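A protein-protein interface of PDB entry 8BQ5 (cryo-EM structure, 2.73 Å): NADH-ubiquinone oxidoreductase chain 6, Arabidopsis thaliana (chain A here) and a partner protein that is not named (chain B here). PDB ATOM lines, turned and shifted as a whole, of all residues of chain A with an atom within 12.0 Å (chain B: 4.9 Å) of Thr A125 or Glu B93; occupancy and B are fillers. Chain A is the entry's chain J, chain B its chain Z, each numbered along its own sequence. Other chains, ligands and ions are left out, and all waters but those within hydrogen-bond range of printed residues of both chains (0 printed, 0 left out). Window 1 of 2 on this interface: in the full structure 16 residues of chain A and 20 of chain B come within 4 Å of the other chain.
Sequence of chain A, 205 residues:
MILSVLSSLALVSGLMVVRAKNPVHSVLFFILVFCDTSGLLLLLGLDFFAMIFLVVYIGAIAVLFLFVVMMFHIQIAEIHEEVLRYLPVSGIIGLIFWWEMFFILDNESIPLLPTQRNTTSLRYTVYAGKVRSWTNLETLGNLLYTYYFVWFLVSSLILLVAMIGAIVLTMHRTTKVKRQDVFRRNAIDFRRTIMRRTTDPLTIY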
ATOM      1  N   THR A 119      25.993  26.308   2.956  1.00  0.00           N
ATOM      2  CA  THR A 119      26.325  27.428   2.035  1.00  0.00           C
ATOM      3  C   THR A 119      26.297  26.920   0.591  1.00  0.00           C
ATOM      4  O   THR A 119      26.668  27.705  -0.309  1.00  0.00           O
ATOM      5  CB  THR A 119      27.682  28.055   2.369  1.00  0.00           C
ATOM      6  OG1 THR A 119      28.681  27.038   2.295  1.00  0.00           O
ATOM      7  CG2 THR A 119      27.706  28.702   3.737  1.00  0.00           C
ATOM      8  N   THR A 120      25.855  25.673   0.380  1.00  0.00           N
ATOM      9  CA  THR A 120      25.851  25.074  -0.985  1.00  0.00           C
ATOM     10  C   THR A 120      24.520  25.381  -1.689  1.00  0.00           C
ATOM     11  O   THR A 120      24.375  24.973  -2.854  1.00  0.00           O
ATOM     12  CB  THR A 120      26.208  23.582  -0.953  1.00  0.00           C
ATOM     13  OG1 THR A 120      25.315  22.904  -0.069  1.00  0.00           O
ATOM     14  CG2 THR A 120      27.637  23.331  -0.528  1.00  0.00           C
ATOM     15  N   SER A 121      23.583  26.040  -1.007  1.00  0.00           N
ATOM     16  CA  SER A 121      22.329  26.492  -1.660  1.00  0.00           C
ATOM     17  C   SER A 121      22.589  27.869  -2.272  1.00  0.00           C
ATOM     18  O   SER A 121      21.837  28.259  -3.176  1.00  0.00           O
ATOM     19  CB  SER A 121      21.211  26.532  -0.670  1.00  0.00           C
ATOM     20  OG  SER A 121      21.500  27.447   0.378  1.00  0.00           O
ATOM     21  N   LEU A 122      23.628  28.573  -1.801  1.00  0.00           N
ATOM     22  CA  LEU A 122      24.011  29.891  -2.367  1.00  0.00           C
ATOM     23  C   LEU A 122      24.785  29.700  -3.678  1.00  0.00           C
ATOM     24  O   LEU A 122      25.418  30.669  -4.118  1.00  0.00           O
ATOM     25  CB  LEU A 122      24.856  30.635  -1.329  1.00  0.00           C
ATOM     26  CG  LEU A 122      24.088  31.175  -0.126  1.00  0.00           C
ATOM     27  CD1 LEU A 122      24.984  32.067   0.717  1.00  0.00           C
ATOM     28  CD2 LEU A 122      22.849  31.934  -0.571  1.00  0.00           C
ATOM     29  N   ARG A 123      24.742  28.504  -4.273  1.00  0.00           N
ATOM     30  CA  ARG A 123      25.376  28.277  -5.596  1.00  0.00           C
ATOM     31  C   ARG A 123      24.425  28.780  -6.683  1.00  0.00           C
ATOM     32  O   ARG A 123      23.386  28.132  -6.901  1.00  0.00           O
ATOM     33  CB  ARG A 123      25.693  26.794  -5.815  1.00  0.00           C
ATOM     34  CG  ARG A 123      26.771  26.243  -4.896  1.00  0.00           C
ATOM     35  CD  ARG A 123      27.062  24.789  -5.207  1.00  0.00           C
ATOM     36  NE  ARG A 123      28.040  24.201  -4.302  1.00  0.00           N
ATOM     37  CZ  ARG A 123      28.378  22.917  -4.294  1.00  0.00           C
ATOM     38  NH1 ARG A 123      27.815  22.079  -5.145  1.00  0.00           N
ATOM     39  NH2 ARG A 123      29.279  22.474  -3.436  1.00  0.00           N
ATOM     40  N   TYR A 124      24.764  29.896  -7.326  1.00  0.00           N
ATOM     41  CA  TYR A 124      23.958  30.398  -8.468  1.00  0.00           C
ATOM     42  C   TYR A 124      24.348  29.612  -9.728  1.00  0.00           C
ATOM     43  O   TYR A 124      25.555  29.449  -9.968  1.00  0.00           O
ATOM     44  CB  TYR A 124      24.195  31.898  -8.611  1.00  0.00           C
ATOM     45  CG  TYR A 124      23.404  32.579  -9.691  1.00  0.00           C
ATOM     46  CD1 TYR A 124      22.022  32.601  -9.656  1.00  0.00           C
ATOM     47  CD2 TYR A 124      24.045  33.209 -10.744  1.00  0.00           C
ATOM     48  CE1 TYR A 124      21.294  33.232 -10.646  1.00  0.00           C
ATOM     49  CE2 TYR A 124      23.330  33.848 -11.740  1.00  0.00           C
ATOM     50  CZ  TYR A 124      21.950  33.855 -11.691  1.00  0.00           C
ATOM     51  OH  TYR A 124      21.256  34.485 -12.676  1.00  0.00           O
ATOM     52  N   THR A 125      23.365  29.175 -10.521  1.00  0.00           N
ATOM     53  CA  THR A 125      23.633  28.354 -11.735  1.00  0.00           C
ATOM     54  C   THR A 125      23.233  29.109 -13.006  1.00  0.00           C
ATOM     55  O   THR A 125      22.077  29.542 -13.106  1.00  0.00           O
ATOM     56  CB  THR A 125      22.924  26.999 -11.642  1.00  0.00           C
ATOM     57  OG1 THR A 125      23.518  26.275 -10.565  1.00  0.00           O
ATOM     58  CG2 THR A 125      23.008  26.180 -12.911  1.00  0.00           C
ATOM     59  N   VAL A 126      24.168  29.257 -13.942  1.00  0.00           N
ATOM     60  CA  VAL A 126      23.909  29.953 -15.195  1.00  0.00           C
ATOM     61  C   VAL A 126      23.830  28.902 -16.293  1.00  0.00           C
ATOM     62  O   VAL A 126      24.812  28.198 -16.562  1.00  0.00           O
ATOM     63  CB  VAL A 126      24.990  30.997 -15.500  1.00  0.00           C
ATOM     64  CG1 VAL A 126      24.608  31.817 -16.721  1.00  0.00           C
ATOM     65  CG2 VAL A 126      25.201  31.894 -14.295  1.00  0.00           C
ATOM     66  N   TYR A 127      22.668  28.793 -16.934  1.00  0.00           N
ATOM     67  CA  TYR A 127      22.486  27.786 -17.968  1.00  0.00           C
ATOM     68  C   TYR A 127      23.015  28.226 -19.325  1.00  0.00           C
ATOM     69  O   TYR A 127      23.096  27.398 -20.237  1.00  0.00           O
ATOM     70  CB  TYR A 127      21.007  27.419 -18.097  1.00  0.00           C
ATOM     71  CG  TYR A 127      20.455  26.722 -16.881  1.00  0.00           C
ATOM     72  CD1 TYR A 127      20.596  25.353 -16.722  1.00  0.00           C
ATOM     73  CD2 TYR A 127      19.793  27.433 -15.893  1.00  0.00           C
ATOM     74  CE1 TYR A 127      20.096  24.713 -15.613  1.00  0.00           C
ATOM     75  CE2 TYR A 127      19.288  26.801 -14.779  1.00  0.00           C
ATOM     76  CZ  TYR A 127      19.442  25.441 -14.645  1.00  0.00           C
ATOM     77  OH  TYR A 127      18.943  24.800 -13.538  1.00  0.00           O
ATOM     78  N   ALA A 128      23.367  29.503 -19.480  1.00  0.00           N
ATOM     79  CA  ALA A 128      23.802  29.992 -20.785  1.00  0.00           C
ATOM     80  C   ALA A 128      25.124  29.360 -21.203  1.00  0.00           C
ATOM     81  O   ALA A 128      25.299  28.983 -22.368  1.00  0.00           O
ATOM     82  CB  ALA A 128      23.910  31.514 -20.763  1.00  0.00           C
ATOM     83  N   GLY A 129      26.062  29.228 -20.270  1.00  0.00           N
ATOM     84  CA  GLY A 129      27.331  28.597 -20.576  1.00  0.00           C
ATOM     85  C   GLY A 129      27.300  27.087 -20.617  1.00  0.00           C
ATOM     86  O   GLY A 129      28.323  26.471 -20.928  1.00  0.00           O
ATOM     87  N   LYS A 130      26.159  26.473 -20.315  1.00  0.00           N
ATOM     88  CA  LYS A 130      26.022  25.025 -20.313  1.00  0.00           C
ATOM     89  C   LYS A 130      25.306  24.492 -21.545  1.00  0.00           C
ATOM     90  O   LYS A 130      25.093  23.281 -21.642  1.00  0.00           O
ATOM     91  CB  LYS A 130      25.273  24.572 -19.058  1.00  0.00           C
ATOM     92  CG  LYS A 130      26.118  24.520 -17.808  1.00  0.00           C
ATOM     93  CD  LYS A 130      25.244  24.310 -16.586  1.00  0.00           C
ATOM     94  CE  LYS A 130      25.958  24.733 -15.318  1.00  0.00           C
ATOM     95  NZ  LYS A 130      26.373  23.562 -14.501  1.00  0.00           N
ATOM     96  N   VAL A 131      24.916  25.362 -22.477  1.00  0.00           N
ATOM     97  CA  VAL A 131      24.189  24.905 -23.657  1.00  0.00           C
ATOM     98  C   VAL A 131      25.099  24.076 -24.552  1.00  0.00           C
ATOM     99  O   VAL A 131      24.724  22.990 -25.011  1.00  0.00           O
ATOM    100  CB  VAL A 131      23.597  26.107 -24.410  1.00  0.00           C
ATOM    101  CG1 VAL A 131      22.974  25.659 -25.719  1.00  0.00           C
ATOM    102  CG2 VAL A 131      22.588  26.826 -23.541  1.00  0.00           C
ATOM    103  N   LEU B  89      14.134  27.925 -17.253  1.00  0.00           N
ATOM    104  CA  LEU B  89      15.069  27.361 -16.287  1.00  0.00           C
ATOM    105  C   LEU B  89      15.834  28.459 -15.560  1.00  0.00           C
ATOM    106  O   LEU B  89      15.990  28.415 -14.333  1.00  0.00           O
ATOM    107  CB  LEU B  89      16.039  26.417 -16.997  1.00  0.00           C
ATOM    108  CG  LEU B  89      15.416  25.227 -17.726  1.00  0.00           C
ATOM    109  CD1 LEU B  89      16.376  24.674 -18.765  1.00  0.00           C
ATOM    110  CD2 LEU B  89      15.031  24.154 -16.731  1.00  0.00           C
ATOM    111  N   GLN B  90      16.306  29.460 -16.305  1.00  0.00           N
ATOM    112  CA  GLN B  90      17.039  30.565 -15.698  1.00  0.00           C
ATOM    113  C   GLN B  90      16.152  31.363 -14.754  1.00  0.00           C
ATOM    114  O   GLN B  90      16.605  31.793 -13.691  1.00  0.00           O
ATOM    115  CB  GLN B  90      17.612  31.475 -16.783  1.00  0.00           C
ATOM    116  CG  GLN B  90      18.831  32.272 -16.348  1.00  0.00           C
ATOM    117  CD  GLN B  90      19.791  31.460 -15.505  1.00  0.00           C
ATOM    118  OE1 GLN B  90      20.411  30.517 -15.992  1.00  0.00           O
ATOM    119  NE2 GLN B  90      19.929  31.830 -14.239  1.00  0.00           N
ATOM    120  N   ALA B  91      14.893  31.591 -15.132  1.00  0.00           N
ATOM    121  CA  ALA B  91      13.982  32.335 -14.269  1.00  0.00           C
ATOM    122  C   ALA B  91      13.739  31.596 -12.962  1.00  0.00           C
ATOM    123  O   ALA B  91      13.754  32.200 -11.879  1.00  0.00           O
ATOM    124  CB  ALA B  91      12.663  32.585 -14.996  1.00  0.00           C
ATOM    125  N   GLU B  92      13.522  30.282 -13.042  1.00  0.00           N
ATOM    126  CA  GLU B  92      13.339  29.492 -11.831  1.00  0.00           C
ATOM    127  C   GLU B  92      14.589  29.536 -10.957  1.00  0.00           C
ATOM    128  O   GLU B  92      14.500  29.687  -9.732  1.00  0.00           O
ATOM    129  CB  GLU B  92      12.985  28.055 -12.202  1.00  0.00           C
ATOM    130  CG  GLU B  92      13.229  27.053 -11.099  1.00  0.00           C
ATOM    131  CD  GLU B  92      13.327  25.645 -11.632  1.00  0.00           C
ATOM    132  OE1 GLU B  92      14.461  25.190 -11.882  1.00  0.00           O
ATOM    133  OE2 GLU B  92      12.274  24.998 -11.809  1.00  0.00           O
ATOM    134  N   GLU B  93      15.761  29.439 -11.582  1.00  0.00           N
ATOM    135  CA  GLU B  93      17.031  29.475 -10.812  1.00  0.00           C
ATOM    136  C   GLU B  93      17.191  30.849 -10.156  1.00  0.00           C
ATOM    137  O   GLU B  93      17.644  30.893  -9.000  1.00  0.00           O
ATOM    138  CB  GLU B  93      18.218  29.134 -11.716  1.00  0.00           C
ATOM    139  CG  GLU B  93      19.571  29.340 -11.061  1.00  0.00           C
ATOM    140  CD  GLU B  93      19.903  28.425  -9.894  1.00  0.00           C
ATOM    141  OE1 GLU B  93      20.636  28.870  -8.991  1.00  0.00           O
ATOM    142  OE2 GLU B  93      19.439  27.267  -9.895  1.00  0.00           O
ATOM    143  N   ASP B  94      16.830  31.917 -10.864  1.00  0.00           N
ATOM    144  CA  ASP B  94      16.938  33.258 -10.300  1.00  0.00           C
ATOM    145  C   ASP B  94      16.032  33.413  -9.088  1.00  0.00           C
ATOM    146  O   ASP B  94      16.443  33.955  -8.056  1.00  0.00           O
ATOM    147  CB  ASP B  94      16.591  34.306 -11.358  1.00  0.00           C
ATOM    148  CG  ASP B  94      17.693  34.499 -12.379  1.00  0.00           C
ATOM    149  OD1 ASP B  94      18.720  33.795 -12.295  1.00  0.00           O
ATOM    150  OD2 ASP B  94      17.535  35.370 -13.260  1.00  0.00           O
ATOM    151  N   GLU B  95      14.786  32.943  -9.199  1.00  0.00           N
ATOM    152  CA  GLU B  95      13.865  33.032  -8.069  1.00  0.00           C
ATOM    153  C   GLU B  95      14.371  32.231  -6.875  1.00  0.00           C
ATOM    154  O   GLU B  95      14.339  32.710  -5.730  1.00  0.00           O
ATOM    155  CB  GLU B  95      12.475  32.553  -8.485  1.00  0.00           C
ATOM    156  CG  GLU B  95      11.447  33.667  -8.642  1.00  0.00           C
ATOM    157  CD  GLU B  95      11.452  34.655  -7.484  1.00  0.00           C
ATOM    158  OE1 GLU B  95      11.696  34.237  -6.331  1.00  0.00           O
ATOM    159  OE2 GLU B  95      11.208  35.854  -7.728  1.00  0.00           O
ATOM    160  N   ARG B  96      14.834  31.010  -7.131  1.00  0.00           N
ATOM    161  CA  ARG B  96      15.382  30.149  -6.051  1.00  0.00           C
ATOM    162  C   ARG B  96      16.567  30.854  -5.382  1.00  0.00           C
ATOM    163  O   ARG B  96      16.617  30.856  -4.150  1.00  0.00           O
ATOM    164  CB  ARG B  96      15.757  28.786  -6.641  1.00  0.00           C
ATOM    165  CG  ARG B  96      16.346  27.789  -5.658  1.00  0.00           C
ATOM    166  CD  ARG B  96      17.463  27.019  -6.334  1.00  0.00           C
ATOM    167  NE  ARG B  96      18.632  27.862  -6.547  1.00  0.00           N
ATOM    168  CZ  ARG B  96      19.586  28.063  -5.647  1.00  0.00           C
ATOM    169  NH1 ARG B  96      19.518  27.471  -4.468  1.00  0.00           N
ATOM    170  NH2 ARG B  96      20.607  28.851  -5.930  1.00  0.00           N
ATOM    171  N   PHE B  97      17.475  31.445  -6.161  1.00  0.00           N
ATOM    172  CA  PHE B  97      18.644  32.077  -5.567  1.00  0.00           C
ATOM    173  C   PHE B  97      18.262  33.326  -4.785  1.00  0.00           C
ATOM    174  O   PHE B  97      18.865  33.613  -3.750  1.00  0.00           O
ATOM    175  CB  PHE B  97      19.680  32.418  -6.634  1.00  0.00           C
ATOM    176  CG  PHE B  97      20.895  33.096  -6.081  1.00  0.00           C
ATOM    177  CD1 PHE B  97      21.926  32.352  -5.537  1.00  0.00           C
ATOM    178  CD2 PHE B  97      21.000  34.474  -6.084  1.00  0.00           C
ATOM    179  CE1 PHE B  97      23.041  32.967  -5.016  1.00  0.00           C
ATOM    180  CE2 PHE B  97      22.112  35.096  -5.565  1.00  0.00           C
ATOM    181  CZ  PHE B  97      23.135  34.340  -5.031  1.00  0.00           C
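NH1 of Arg B96 sits at hydrogen-bond distance from O of Ser A121.
The backbone carbonyl oxygen of Arg A123 is in hydrogen-bond range of the guanidinium group of Arg B96 (3.0 Å).
The side-chain amide nitrogen of Gln B90 sits at hydrogen-bond distance from the side-chain hydroxyl of Tyr A124, 3.4 Å away.
OD1 of Asp B94 sits at hydrogen-bond distance from OH of Tyr A124, at 2.7 Å.
The backbone carbonyl oxygen (O) of Thr A125 lies within hydrogen-bond range of the side-chain amide nitrogen (NE2) of Gln B90.
The side-chain carboxylate of Glu B93 is in hydrogen-bond range of the backbone NH of Thr A125 (3.1 Å).
The backbone NH (N) of Tyr A127 is in hydrogen-bond range of the side-chain amide oxygen (OE1) of Gln B90 (3.0 Å).
Of the 9 printed residues of chain B, 6 touch a printed residue of chain A.
Printed residues of chain B that touch a printed residue of chain A: Leu B89, Gln B90, Glu B93, Asp B94, Arg B96 and Phe B97.
Among the printed residues, 14 pairs touch across the chains.
Among the printed residues, no Asp or Glu carboxylate lies within 4 Å of a Lys or Arg side-chain nitrogen of the other chain.
Among the printed residues, merely in contact across the chains: Leu A122 with Phe B97 (3.4 Å), Arg A123 with Glu B93 (3.5 Å), Tyr A124 with Glu B93 (3.7 Å), Tyr A124 with Phe B97 (3.8 Å), Val A126 with Gln B90 (3.6 Å), Tyr A127 with Leu B89 (3.7 Å) and Tyr A127 with Glu B93 (3.996 Å).
Thr A120 touches none of the printed residues of chain B.
Of the printed residues of chain B, Leu A122 touches Phe B97.
Printed residues of chain B within 4 Å of Arg A123: Glu B93 (3.5 Å) and Arg B96 (3.0 Å).
Thr A125 touches just these residues of chain B: Gln B90 and Glu B93.
Gln B90 touches just these residues of chain A: Tyr A124, Thr A125, Val A126 and Tyr A127.
No residue of chain A comes within 4 Å of Ala B91.
No residue of chain A comes within 4 Å of Glu B92.
Printed residues of chain A within 4 Å of Glu B93: Arg A123 (3.5 Å), Tyr A124 (3.7 Å), Thr A125 (3.1 Å) and Tyr A127 (3.996 Å).
Of chain A, only Tyr A124 (2.7 Å) comes within 4 Å of Asp B94.
Printed residues of chain A within 4 Å of Arg B96: Ser A121 (2.8 Å) and Arg A123 (3.0 Å).
Of chain A, only Leu A122 and Tyr A124 come within 4 Å of Phe B97.
The nearest printed residue of chain B that does not touch Thr A125 is Arg B96 (5.4 Å).
The nearest printed residue of chain A that does not touch Glu B93 is Val A126 (5.4 Å).
The nearest printed residue of chain B that does not touch Arg A123 is Phe B97 (4.5 Å).
NE2 of Gln B90 sits at hydrogen-bond distance from OD1 of Asp B94.
The side-chain carboxylate of Glu B93 is in salt-bridge range of the guanidinium group of Arg B96, 3.1 Å away.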
